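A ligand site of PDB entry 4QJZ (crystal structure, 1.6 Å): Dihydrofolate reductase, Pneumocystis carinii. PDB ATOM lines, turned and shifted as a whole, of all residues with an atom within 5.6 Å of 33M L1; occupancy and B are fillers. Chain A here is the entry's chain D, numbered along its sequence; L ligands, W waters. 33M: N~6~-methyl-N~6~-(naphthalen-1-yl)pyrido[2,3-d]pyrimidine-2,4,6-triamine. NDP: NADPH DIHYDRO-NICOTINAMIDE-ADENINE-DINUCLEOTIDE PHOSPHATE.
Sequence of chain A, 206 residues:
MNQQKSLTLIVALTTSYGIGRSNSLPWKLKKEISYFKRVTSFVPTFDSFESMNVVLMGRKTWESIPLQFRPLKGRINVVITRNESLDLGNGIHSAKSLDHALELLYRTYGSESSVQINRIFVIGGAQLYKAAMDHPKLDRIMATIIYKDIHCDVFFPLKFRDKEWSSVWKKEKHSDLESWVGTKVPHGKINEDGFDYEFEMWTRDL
The side-chain carboxylate (OE2) of Glu 32 is in hydrogen-bond range of a nitrogen (NAB) of 33M L1. The backbone carbonyl oxygen (O) of Ile 10 sits at hydrogen-bond distance from a nitrogen (NAC) of 33M L1 (2.9 Å). The backbone carbonyl oxygen (O) of Ile 123 sits at hydrogen-bond distance from a nitrogen (NAC) of 33M L1. The side-chain hydroxyl (OH) of Tyr 129 is in hydrogen-bond range of a nitrogen (NAC) of 33M L1. A nitrogen (N1) of 33M L1 sits at hydrogen-bond distance from the backbone NH (N) of Val 11 (3.4 Å). An oxygen (O7N) of NDP L2 is in hydrogen-bond range of the side-chain hydroxyl of Tyr 129 (3.4 Å). N of Thr 61 lies within hydrogen-bond range of O2A of NDP L2 (2.9 Å). OG1 of Thr 61 lies within hydrogen-bond range of O2A of NDP L2, 2.7 Å away. The backbone NH (N) of Ala 12 sits at hydrogen-bond distance from an oxygen (O7N) of NDP L2, at 3.0 Å. A nitrogen (N7N) of NDP L2 sits at hydrogen-bond distance from the backbone carbonyl oxygen of Ala 12, at 2.8 Å. N of Leu 25 is in hydrogen-bond range of O2D of NDP L2, at 3.5 Å.
Water W4 bridges the side-chain carboxylate (OE1) of Glu 32 (2.8 Å) and a nitrogen (NAM) of 33M L1 (3.1 Å). Water W3 lies within hydrogen-bond range of OG1 of Thr 144 (2.8 Å), O of Met 142 (2.9 Å), O of Val 11 (3.2 Å) and NAB of 33M L1 (3.4 Å). Water W2 bridges an oxygen (O2D) of NDP L2 (2.4 Å) and the side-chain hydroxyl (OG) of Ser 64 (2.7 Å).
The side-chain carboxylate of Glu 32 is in hydrogen-bond range of the side-chain hydroxyl of Thr 144, at 2.7 Å. O of Ile 10 sits at hydrogen-bond distance from OH of Tyr 129 (2.7 Å). N of Ile 10 sits at hydrogen-bond distance from O of Val 122, 3.0 Å away. The backbone carbonyl oxygen (O) of Ile 123 is in hydrogen-bond range of the side-chain hydroxyl (OH) of Tyr 129 (3.3 Å). N of Thr 144 lies within hydrogen-bond range of O of Val 11 (2.7 Å). N of Val 11 is in hydrogen-bond range of O of Met 142, at 2.9 Å. The side-chain hydroxyl of Ser 64 sits at hydrogen-bond distance from the backbone carbonyl oxygen of Thr 61 (2.7 Å).
Residues that only touch 33M L1: Ala 12 (3.6 Å), Leu 25 (3.7 Å), Ile 33 (3.5 Å), Phe 36 (3.3 Å), Thr 61 (3.6 Å), Pro 66 (3.7 Å), Leu 72 (3.9 Å) and Thr 144 (3.6 Å). Hydrophobic or aromatic side chains that line 33M L1: Ile 10, Ala 12, Leu 25, Ile 33, Phe 36, Pro 66, Leu 72 and Ile 123. Within 4 Å of 33M L1: Ile 10, Val 11, Ala 12, Leu 25, Glu 32, Ile 33, Phe 36, Thr 61, Pro 66, Leu 72, Ile 123, Tyr 129 and Thr 144.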
ATOM      1  N   ILE A  10       6.347  18.805  16.054  1.00  0.00           N
ATOM      2  CA  ILE A  10       7.086  18.896  17.359  1.00  0.00           C
ATOM      3  C   ILE A  10       7.118  17.454  17.963  1.00  0.00           C
ATOM      4  O   ILE A  10       6.101  16.762  17.990  1.00  0.00           O
ATOM      5  CB  ILE A  10       6.489  19.986  18.304  1.00  0.00           C
ATOM      6  CG1 ILE A  10       7.267  20.027  19.656  1.00  0.00           C
ATOM      7  CG2 ILE A  10       5.016  19.779  18.596  1.00  0.00           C
ATOM      8  CD1 ILE A  10       7.105  21.335  20.449  1.00  0.00           C
ATOM      9  N   VAL A  11       8.318  17.075  18.439  1.00  0.00           N
ATOM     10  CA  VAL A  11       8.577  15.691  18.866  1.00  0.00           C
ATOM     11  C   VAL A  11       9.727  15.682  19.903  1.00  0.00           C
ATOM     12  O   VAL A  11      10.629  16.538  19.875  1.00  0.00           O
ATOM     13  CB  VAL A  11       8.891  14.780  17.646  1.00  0.00           C
ATOM     14  CG1 VAL A  11      10.190  15.152  16.923  1.00  0.00           C
ATOM     15  CG2 VAL A  11       8.917  13.300  18.092  1.00  0.00           C
ATOM     16  N   ALA A  12       9.607  14.763  20.866  1.00  0.00           N
ATOM     17  CA  ALA A  12      10.743  14.415  21.728  1.00  0.00           C
ATOM     18  C   ALA A  12      11.162  13.024  21.365  1.00  0.00           C
ATOM     19  O   ALA A  12      10.295  12.129  21.248  1.00  0.00           O
ATOM     20  CB  ALA A  12      10.338  14.441  23.207  1.00  0.00           C
ATOM     21  N   LEU A  25       4.650   7.732  26.742  1.00  0.00           N
ATOM     22  CA  LEU A  25       6.002   8.237  26.563  1.00  0.00           C
ATOM     23  C   LEU A  25       6.940   7.364  27.368  1.00  0.00           C
ATOM     24  O   LEU A  25       6.515   6.910  28.441  1.00  0.00           O
ATOM     25  CB  LEU A  25       6.022   9.697  27.053  1.00  0.00           C
ATOM     26  CG  LEU A  25       5.105  10.609  26.205  1.00  0.00           C
ATOM     27  CD1 LEU A  25       5.156  11.994  26.773  1.00  0.00           C
ATOM     28  CD2 LEU A  25       5.622  10.673  24.780  1.00  0.00           C
ATOM     29  N   GLU A  32      10.120  19.408  30.000  1.00  0.00           N
ATOM     30  CA  GLU A  32       9.994  19.101  28.574  1.00  0.00           C
ATOM     31  C   GLU A  32       8.530  19.349  28.181  1.00  0.00           C
ATOM     32  O   GLU A  32       8.264  20.017  27.184  1.00  0.00           O
ATOM     33  CB  GLU A  32      10.483  17.656  28.247  1.00  0.00           C
ATOM     34  CG  GLU A  32      10.923  17.549  26.788  1.00  0.00           C
ATOM     35  CD  GLU A  32       9.811  17.608  25.762  1.00  0.00           C
ATOM     36  OE1 GLU A  32       8.760  16.966  25.952  1.00  0.00           O
ATOM     37  OE2 GLU A  32      10.043  18.239  24.681  1.00  0.00           O
ATOM     38  N   ILE A  33       7.562  18.862  28.970  1.00  0.00           N
ATOM     39  CA  ILE A  33       6.158  19.213  28.685  1.00  0.00           C
ATOM     40  C   ILE A  33       5.850  20.688  28.712  1.00  0.00           C
ATOM     41  O   ILE A  33       5.078  21.127  27.952  1.00  0.00           O
ATOM     42  CB  ILE A  33       5.176  18.441  29.545  1.00  0.00           C
ATOM     43  CG1 ILE A  33       5.512  16.958  29.412  1.00  0.00           C
ATOM     44  CG2 ILE A  33       3.754  18.817  29.168  1.00  0.00           C
ATOM     45  CD1 ILE A  33       4.447  16.156  28.756  1.00  0.00           C
ATOM     46  N   TYR A  35       7.869  23.063  27.872  1.00  0.00           N
ATOM     47  CA  TYR A  35       8.420  23.583  26.634  1.00  0.00           C
ATOM     48  C   TYR A  35       7.450  23.242  25.519  1.00  0.00           C
ATOM     49  O   TYR A  35       7.130  24.097  24.711  1.00  0.00           O
ATOM     50  CB  TYR A  35       9.790  22.957  26.342  1.00  0.00           C
ATOM     51  CG  TYR A  35      10.295  23.251  24.937  1.00  0.00           C
ATOM     52  CD1 TYR A  35      10.893  24.485  24.675  1.00  0.00           C
ATOM     53  CD2 TYR A  35      10.200  22.290  23.882  1.00  0.00           C
ATOM     54  CE1 TYR A  35      11.410  24.802  23.425  1.00  0.00           C
ATOM     55  CE2 TYR A  35      10.750  22.606  22.606  1.00  0.00           C
ATOM     56  CZ  TYR A  35      11.315  23.850  22.401  1.00  0.00           C
ATOM     57  OH  TYR A  35      11.899  24.221  21.194  1.00  0.00           O
ATOM     58  N   PHE A  36       6.983  21.982  25.474  1.00  0.00           N
ATOM     59  CA  PHE A  36       5.994  21.630  24.442  1.00  0.00           C
ATOM     60  C   PHE A  36       4.775  22.582  24.554  1.00  0.00           C
ATOM     61  O   PHE A  36       4.323  23.059  23.566  1.00  0.00           O
ATOM     62  CB  PHE A  36       5.525  20.181  24.655  1.00  0.00           C
ATOM     63  CG  PHE A  36       4.254  19.801  23.927  1.00  0.00           C
ATOM     64  CD1 PHE A  36       4.321  19.308  22.615  1.00  0.00           C
ATOM     65  CD2 PHE A  36       3.019  19.847  24.605  1.00  0.00           C
ATOM     66  CE1 PHE A  36       3.170  18.890  21.959  1.00  0.00           C
ATOM     67  CE2 PHE A  36       1.840  19.431  23.924  1.00  0.00           C
ATOM     68  CZ  PHE A  36       1.922  18.974  22.634  1.00  0.00           C
ATOM     69  N   THR A  61      -2.548   8.946  20.240  1.00  0.00           N
ATOM     70  CA  THR A  61      -2.025  10.042  21.043  1.00  0.00           C
ATOM     71  C   THR A  61      -3.100  10.733  21.878  1.00  0.00           C
ATOM     72  O   THR A  61      -2.844  11.031  23.057  1.00  0.00           O
ATOM     73  CB  THR A  61      -1.238  11.034  20.182  1.00  0.00           C
ATOM     74  OG1 THR A  61      -0.163  10.291  19.619  1.00  0.00           O
ATOM     75  CG2 THR A  61      -0.665  12.186  20.991  1.00  0.00           C
ATOM     76  N   SER A  64      -3.904   8.716  24.659  1.00  0.00           N
ATOM     77  CA  SER A  64      -2.806   8.594  25.595  1.00  0.00           C
ATOM     78  C   SER A  64      -2.748   9.779  26.565  1.00  0.00           C
ATOM     79  O   SER A  64      -2.102   9.683  27.602  1.00  0.00           O
ATOM     80  CB  SER A  64      -1.448   8.415  24.859  1.00  0.00           C
ATOM     81  OG  SER A  64      -0.957   9.657  24.437  1.00  0.00           O
ATOM     82  N   ILE A  65      -3.374  10.906  26.240  1.00  0.00           N
ATOM     83  CA  ILE A  65      -3.209  12.083  27.112  1.00  0.00           C
ATOM     84  C   ILE A  65      -4.141  11.880  28.336  1.00  0.00           C
ATOM     85  O   ILE A  65      -5.354  11.849  28.157  1.00  0.00           O
ATOM     86  CB  ILE A  65      -3.548  13.376  26.346  1.00  0.00           C
ATOM     87  CG1 ILE A  65      -2.602  13.540  25.124  1.00  0.00           C
ATOM     88  CG2 ILE A  65      -3.552  14.636  27.227  1.00  0.00           C
ATOM     89  CD1 ILE A  65      -2.840  14.827  24.346  1.00  0.00           C
ATOM     90  N   PRO A  66      -3.600  11.732  29.563  1.00  0.00           N
ATOM     91  CA  PRO A  66      -4.573  11.662  30.682  1.00  0.00           C
ATOM     92  C   PRO A  66      -5.650  12.724  30.524  1.00  0.00           C
ATOM     93  O   PRO A  66      -5.382  13.861  30.113  1.00  0.00           O
ATOM     94  CB  PRO A  66      -3.719  11.930  31.953  1.00  0.00           C
ATOM     95  CG  PRO A  66      -2.293  11.699  31.548  1.00  0.00           C
ATOM     96  CD  PRO A  66      -2.225  12.013  30.049  1.00  0.00           C
ATOM     97  N   PHE A  69      -5.516  16.434  31.252  1.00  0.00           N
ATOM     98  CA  PHE A  69      -4.804  17.352  30.387  1.00  0.00           C
ATOM     99  C   PHE A  69      -5.332  17.493  28.966  1.00  0.00           C
ATOM    100  O   PHE A  69      -4.737  18.213  28.138  1.00  0.00           O
ATOM    101  CB  PHE A  69      -3.301  17.055  30.431  1.00  0.00           C
ATOM    102  CG  PHE A  69      -2.749  17.103  31.826  1.00  0.00           C
ATOM    103  CD1 PHE A  69      -2.758  18.313  32.533  1.00  0.00           C
ATOM    104  CD2 PHE A  69      -2.294  15.939  32.443  1.00  0.00           C
ATOM    105  CE1 PHE A  69      -2.290  18.367  33.841  1.00  0.00           C
ATOM    106  CE2 PHE A  69      -1.827  15.991  33.765  1.00  0.00           C
ATOM    107  CZ  PHE A  69      -1.825  17.196  34.451  1.00  0.00           C
ATOM    108  N   LEU A  72      -5.913  19.942  24.929  1.00  0.00           N
ATOM    109  CA  LEU A  72      -4.813  20.818  25.283  1.00  0.00           C
ATOM    110  C   LEU A  72      -5.309  22.244  25.255  1.00  0.00           C
ATOM    111  O   LEU A  72      -5.771  22.761  24.215  1.00  0.00           O
ATOM    112  CB  LEU A  72      -3.603  20.568  24.335  1.00  0.00           C
ATOM    113  CG  LEU A  72      -3.152  19.082  24.285  1.00  0.00           C
ATOM    114  CD1 LEU A  72      -2.062  18.796  23.232  1.00  0.00           C
ATOM    115  CD2 LEU A  72      -2.667  18.540  25.625  1.00  0.00           C
ATOM    116  N   VAL A 122       1.935  19.533  14.172  1.00  0.00           N
ATOM    117  CA  VAL A 122       1.665  18.080  14.305  1.00  0.00           C
ATOM    118  C   VAL A 122       2.357  17.560  15.533  1.00  0.00           C
ATOM    119  O   VAL A 122       3.607  17.710  15.750  1.00  0.00           O
ATOM    120  CB  VAL A 122       2.206  17.360  13.072  1.00  0.00           C
ATOM    121  CG1 VAL A 122       2.010  15.854  13.189  1.00  0.00           C
ATOM    122  CG2 VAL A 122       1.445  17.889  11.852  1.00  0.00           C
ATOM    123  N   ILE A 123       1.576  16.968  16.427  1.00  0.00           N
ATOM    124  CA  ILE A 123       2.182  16.590  17.755  1.00  0.00           C
ATOM    125  C   ILE A 123       2.296  15.066  18.031  1.00  0.00           C
ATOM    126  O   ILE A 123       2.597  14.671  19.188  1.00  0.00           O
ATOM    127  CB  ILE A 123       1.416  17.286  18.954  1.00  0.00           C
ATOM    128  CG1 ILE A 123       0.043  16.593  19.109  1.00  0.00           C
ATOM    129  CG2 ILE A 123       1.314  18.831  18.710  1.00  0.00           C
ATOM    130  CD1 ILE A 123      -0.634  16.865  20.461  1.00  0.00           C
ATOM    131  N   GLY A 124       2.094  14.198  17.001  1.00  0.00           N
ATOM    132  CA  GLY A 124       2.297  12.731  17.159  1.00  0.00           C
ATOM    133  C   GLY A 124       1.006  12.002  16.843  1.00  0.00           C
ATOM    134  O   GLY A 124       0.048  12.654  16.592  1.00  0.00           O
ATOM    135  N   TYR A 129       2.930  11.214  12.292  1.00  0.00           N
ATOM    136  CA  TYR A 129       4.224  11.821  11.906  1.00  0.00           C
ATOM    137  C   TYR A 129       4.657  11.295  10.526  1.00  0.00           C
ATOM    138  O   TYR A 129       5.336  12.011   9.770  1.00  0.00           O
ATOM    139  CB  TYR A 129       5.337  11.441  12.854  1.00  0.00           C
ATOM    140  CG  TYR A 129       5.369  12.119  14.226  1.00  0.00           C
ATOM    141  CD1 TYR A 129       5.075  13.487  14.353  1.00  0.00           C
ATOM    142  CD2 TYR A 129       5.713  11.399  15.417  1.00  0.00           C
ATOM    143  CE1 TYR A 129       5.165  14.155  15.607  1.00  0.00           C
ATOM    144  CE2 TYR A 129       5.806  12.024  16.665  1.00  0.00           C
ATOM    145  CZ  TYR A 129       5.502  13.447  16.778  1.00  0.00           C
ATOM    146  OH  TYR A 129       5.601  14.095  18.008  1.00  0.00           O
ATOM    147  N   MET A 142      10.521  20.767  15.510  1.00  0.00           N
ATOM    148  CA  MET A 142      10.993  21.207  16.847  1.00  0.00           C
ATOM    149  C   MET A 142      11.283  19.907  17.571  1.00  0.00           C
ATOM    150  O   MET A 142      10.348  19.114  17.901  1.00  0.00           O
ATOM    151  CB  MET A 142       9.897  22.027  17.578  1.00  0.00           C
ATOM    152  CG  MET A 142       9.318  23.203  16.748  1.00  0.00           C
ATOM    153  SD  MET A 142      10.593  24.334  16.196  1.00  0.00           S
ATOM    154  CE  MET A 142      11.241  24.929  17.697  1.00  0.00           C
ATOM    155  N   THR A 144      13.104  17.532  20.475  1.00  0.00           N
ATOM    156  CA  THR A 144      13.785  17.458  21.777  1.00  0.00           C
ATOM    157  C   THR A 144      14.593  16.203  21.706  1.00  0.00           C
ATOM    158  O   THR A 144      13.991  15.109  21.657  1.00  0.00           O
ATOM    159  CB  THR A 144      12.796  17.423  22.921  1.00  0.00           C
ATOM    160  OG1 THR A 144      12.085  18.670  22.908  1.00  0.00           O
ATOM    161  CG2 THR A 144      13.513  17.422  24.317  1.00  0.00           C
HETATM  162  CAL 33M L   1       3.657  15.362  22.968  1.00  0.00           C
HETATM  163  C5  33M L   1       4.912  15.966  22.808  1.00  0.00           C
HETATM  164  C6  33M L   1       5.447  16.372  21.530  1.00  0.00           C
HETATM  165  NAC 33M L   1       4.734  16.176  20.435  1.00  0.00           N
HETATM  166  N1  33M L   1       6.648  16.982  21.430  1.00  0.00           N
HETATM  167  C2  33M L   1       7.402  17.137  22.552  1.00  0.00           C
HETATM  168  NAB 33M L   1       8.618  17.757  22.556  1.00  0.00           N
HETATM  169  N3  33M L   1       6.942  16.716  23.764  1.00  0.00           N
HETATM  170  C4  33M L   1       5.714  16.158  23.926  1.00  0.00           C
HETATM  171  NAM 33M L   1       5.347  15.830  25.190  1.00  0.00           N
HETATM  172  CAK 33M L   1       4.111  15.222  25.352  1.00  0.00           C
HETATM  173  CAR 33M L   1       3.238  15.002  24.294  1.00  0.00           C
HETATM  174  NAX 33M L   1       2.014  14.443  24.543  1.00  0.00           N
HETATM  175  CAA 33M L   1       1.099  14.156  23.363  1.00  0.00           C
HETATM  176  CAS 33M L   1       1.607  14.137  25.842  1.00  0.00           C
HETATM  177  CAV 33M L   1       1.192  15.184  26.699  1.00  0.00           C
HETATM  178  CAJ 33M L   1       1.144  16.553  26.284  1.00  0.00           C
HETATM  179  CAE 33M L   1       0.767  17.581  27.127  1.00  0.00           C
HETATM  180  CAD 33M L   1       0.385  17.252  28.454  1.00  0.00           C
HETATM  181  CAH 33M L   1       0.386  15.914  28.898  1.00  0.00           C
HETATM  182  CAT 33M L   1       0.790  14.863  28.032  1.00  0.00           C
HETATM  183  CAI 33M L   1       0.812  13.546  28.510  1.00  0.00           C
HETATM  184  CAF 33M L   1       1.253  12.525  27.646  1.00  0.00           C
HETATM  185  CAG 33M L   1       1.600  12.815  26.287  1.00  0.00           C
HETATM  186  PA  NDP L   2      -1.118   7.902  16.512  1.00  0.00           P
HETATM  187  O1A NDP L   2      -0.395   8.216  15.218  1.00  0.00           O
HETATM  188  O2A NDP L   2      -1.152   8.805  17.652  1.00  0.00           O
HETATM  189  O5B NDP L   2      -2.641   7.491  16.213  1.00  0.00           O
HETATM  190  C5B NDP L   2      -2.805   6.444  15.211  1.00  0.00           C
HETATM  191  C4B NDP L   2      -4.276   6.469  14.941  1.00  0.00           C
HETATM  192  O4B NDP L   2      -4.524   7.788  14.498  1.00  0.00           O
HETATM  193  C3B NDP L   2      -4.702   5.558  13.817  1.00  0.00           C
HETATM  194  O3B NDP L   2      -5.118   4.307  14.440  1.00  0.00           O
HETATM  195  C2B NDP L   2      -5.859   6.315  13.216  1.00  0.00           C
HETATM  196  O2B NDP L   2      -6.987   6.462  14.050  1.00  0.00           O
HETATM  197  C1B NDP L   2      -5.332   7.757  13.288  1.00  0.00           C
HETATM  198  N9A NDP L   2      -4.345   8.165  12.222  1.00  0.00           N
HETATM  199  C8A NDP L   2      -3.044   8.479  12.404  1.00  0.00           C
HETATM  200  N7A NDP L   2      -2.553   8.848  11.217  1.00  0.00           N
HETATM  201  C5A NDP L   2      -3.570   8.810  10.330  1.00  0.00           C
HETATM  202  C6A NDP L   2      -3.664   9.102   9.027  1.00  0.00           C
HETATM  203  N6A NDP L   2      -2.547   9.512   8.385  1.00  0.00           N
HETATM  204  N1A NDP L   2      -4.807   8.955   8.348  1.00  0.00           N
HETATM  205  C2A NDP L   2      -5.976   8.540   8.984  1.00  0.00           C
HETATM  206  N3A NDP L   2      -5.867   8.227  10.314  1.00  0.00           N
HETATM  207  C4A NDP L   2      -4.672   8.369  10.969  1.00  0.00           C
HETATM  208  O3  NDP L   2      -0.410   6.527  17.073  1.00  0.00           O
HETATM  209  PN  NDP L   2       0.868   5.714  17.031  1.00  0.00           P
HETATM  210  O1N NDP L   2       1.582   5.798  15.730  1.00  0.00           O
HETATM  211  O2N NDP L   2       0.676   4.321  17.597  1.00  0.00           O
HETATM  212  O5D NDP L   2       1.743   6.486  18.087  1.00  0.00           O
HETATM  213  C5D NDP L   2       1.385   6.451  19.497  1.00  0.00           C
HETATM  214  C4D NDP L   2       2.729   6.438  20.244  1.00  0.00           C
HETATM  215  O4D NDP L   2       3.349   7.661  19.940  1.00  0.00           O
HETATM  216  C3D NDP L   2       2.563   6.426  21.850  1.00  0.00           C
HETATM  217  O3D NDP L   2       3.576   5.589  22.417  1.00  0.00           O
HETATM  218  C2D NDP L   2       2.655   7.901  22.227  1.00  0.00           C
HETATM  219  O2D NDP L   2       3.033   8.089  23.690  1.00  0.00           O
HETATM  220  C1D NDP L   2       3.842   8.221  21.277  1.00  0.00           C
HETATM  221  N1N NDP L   2       4.027   9.684  21.079  1.00  0.00           N
HETATM  222  C2N NDP L   2       5.283  10.245  21.344  1.00  0.00           C
HETATM  223  C3N NDP L   2       5.464  11.612  21.118  1.00  0.00           C
HETATM  224  C7N NDP L   2       6.741  12.160  21.354  1.00  0.00           C
HETATM  225  O7N NDP L   2       6.999  13.341  21.035  1.00  0.00           O
HETATM  226  N7N NDP L   2       7.669  11.348  21.894  1.00  0.00           N
HETATM  227  C4N NDP L   2       4.380  12.441  20.794  1.00  0.00           C
HETATM  228  C5N NDP L   2       3.096  11.877  20.483  1.00  0.00           C
HETATM  229  C6N NDP L   2       2.938  10.523  20.700  1.00  0.00           C
HETATM  230  P2B NDP L   2      -8.363   5.440  14.048  1.00  0.00           P
HETATM  231  O1X NDP L   2      -8.903   5.480  12.553  1.00  0.00           O
HETATM  232  O2X NDP L   2      -7.666   4.093  14.281  1.00  0.00           O
HETATM  233  O3X NDP L   2      -9.240   5.907  15.121  1.00  0.00           O
HETATM  234  O   HOH W   1       3.236  10.553  29.599  1.00  0.00           O
HETATM  235  O   HOH W   2       1.670   9.550  25.094  1.00  0.00           O
HETATM  236  O   HOH W   3      10.705  19.671  20.725  1.00  0.00           O
HETATM  237  O   HOH W   4       7.605  14.632  26.894  1.00  0.00           O
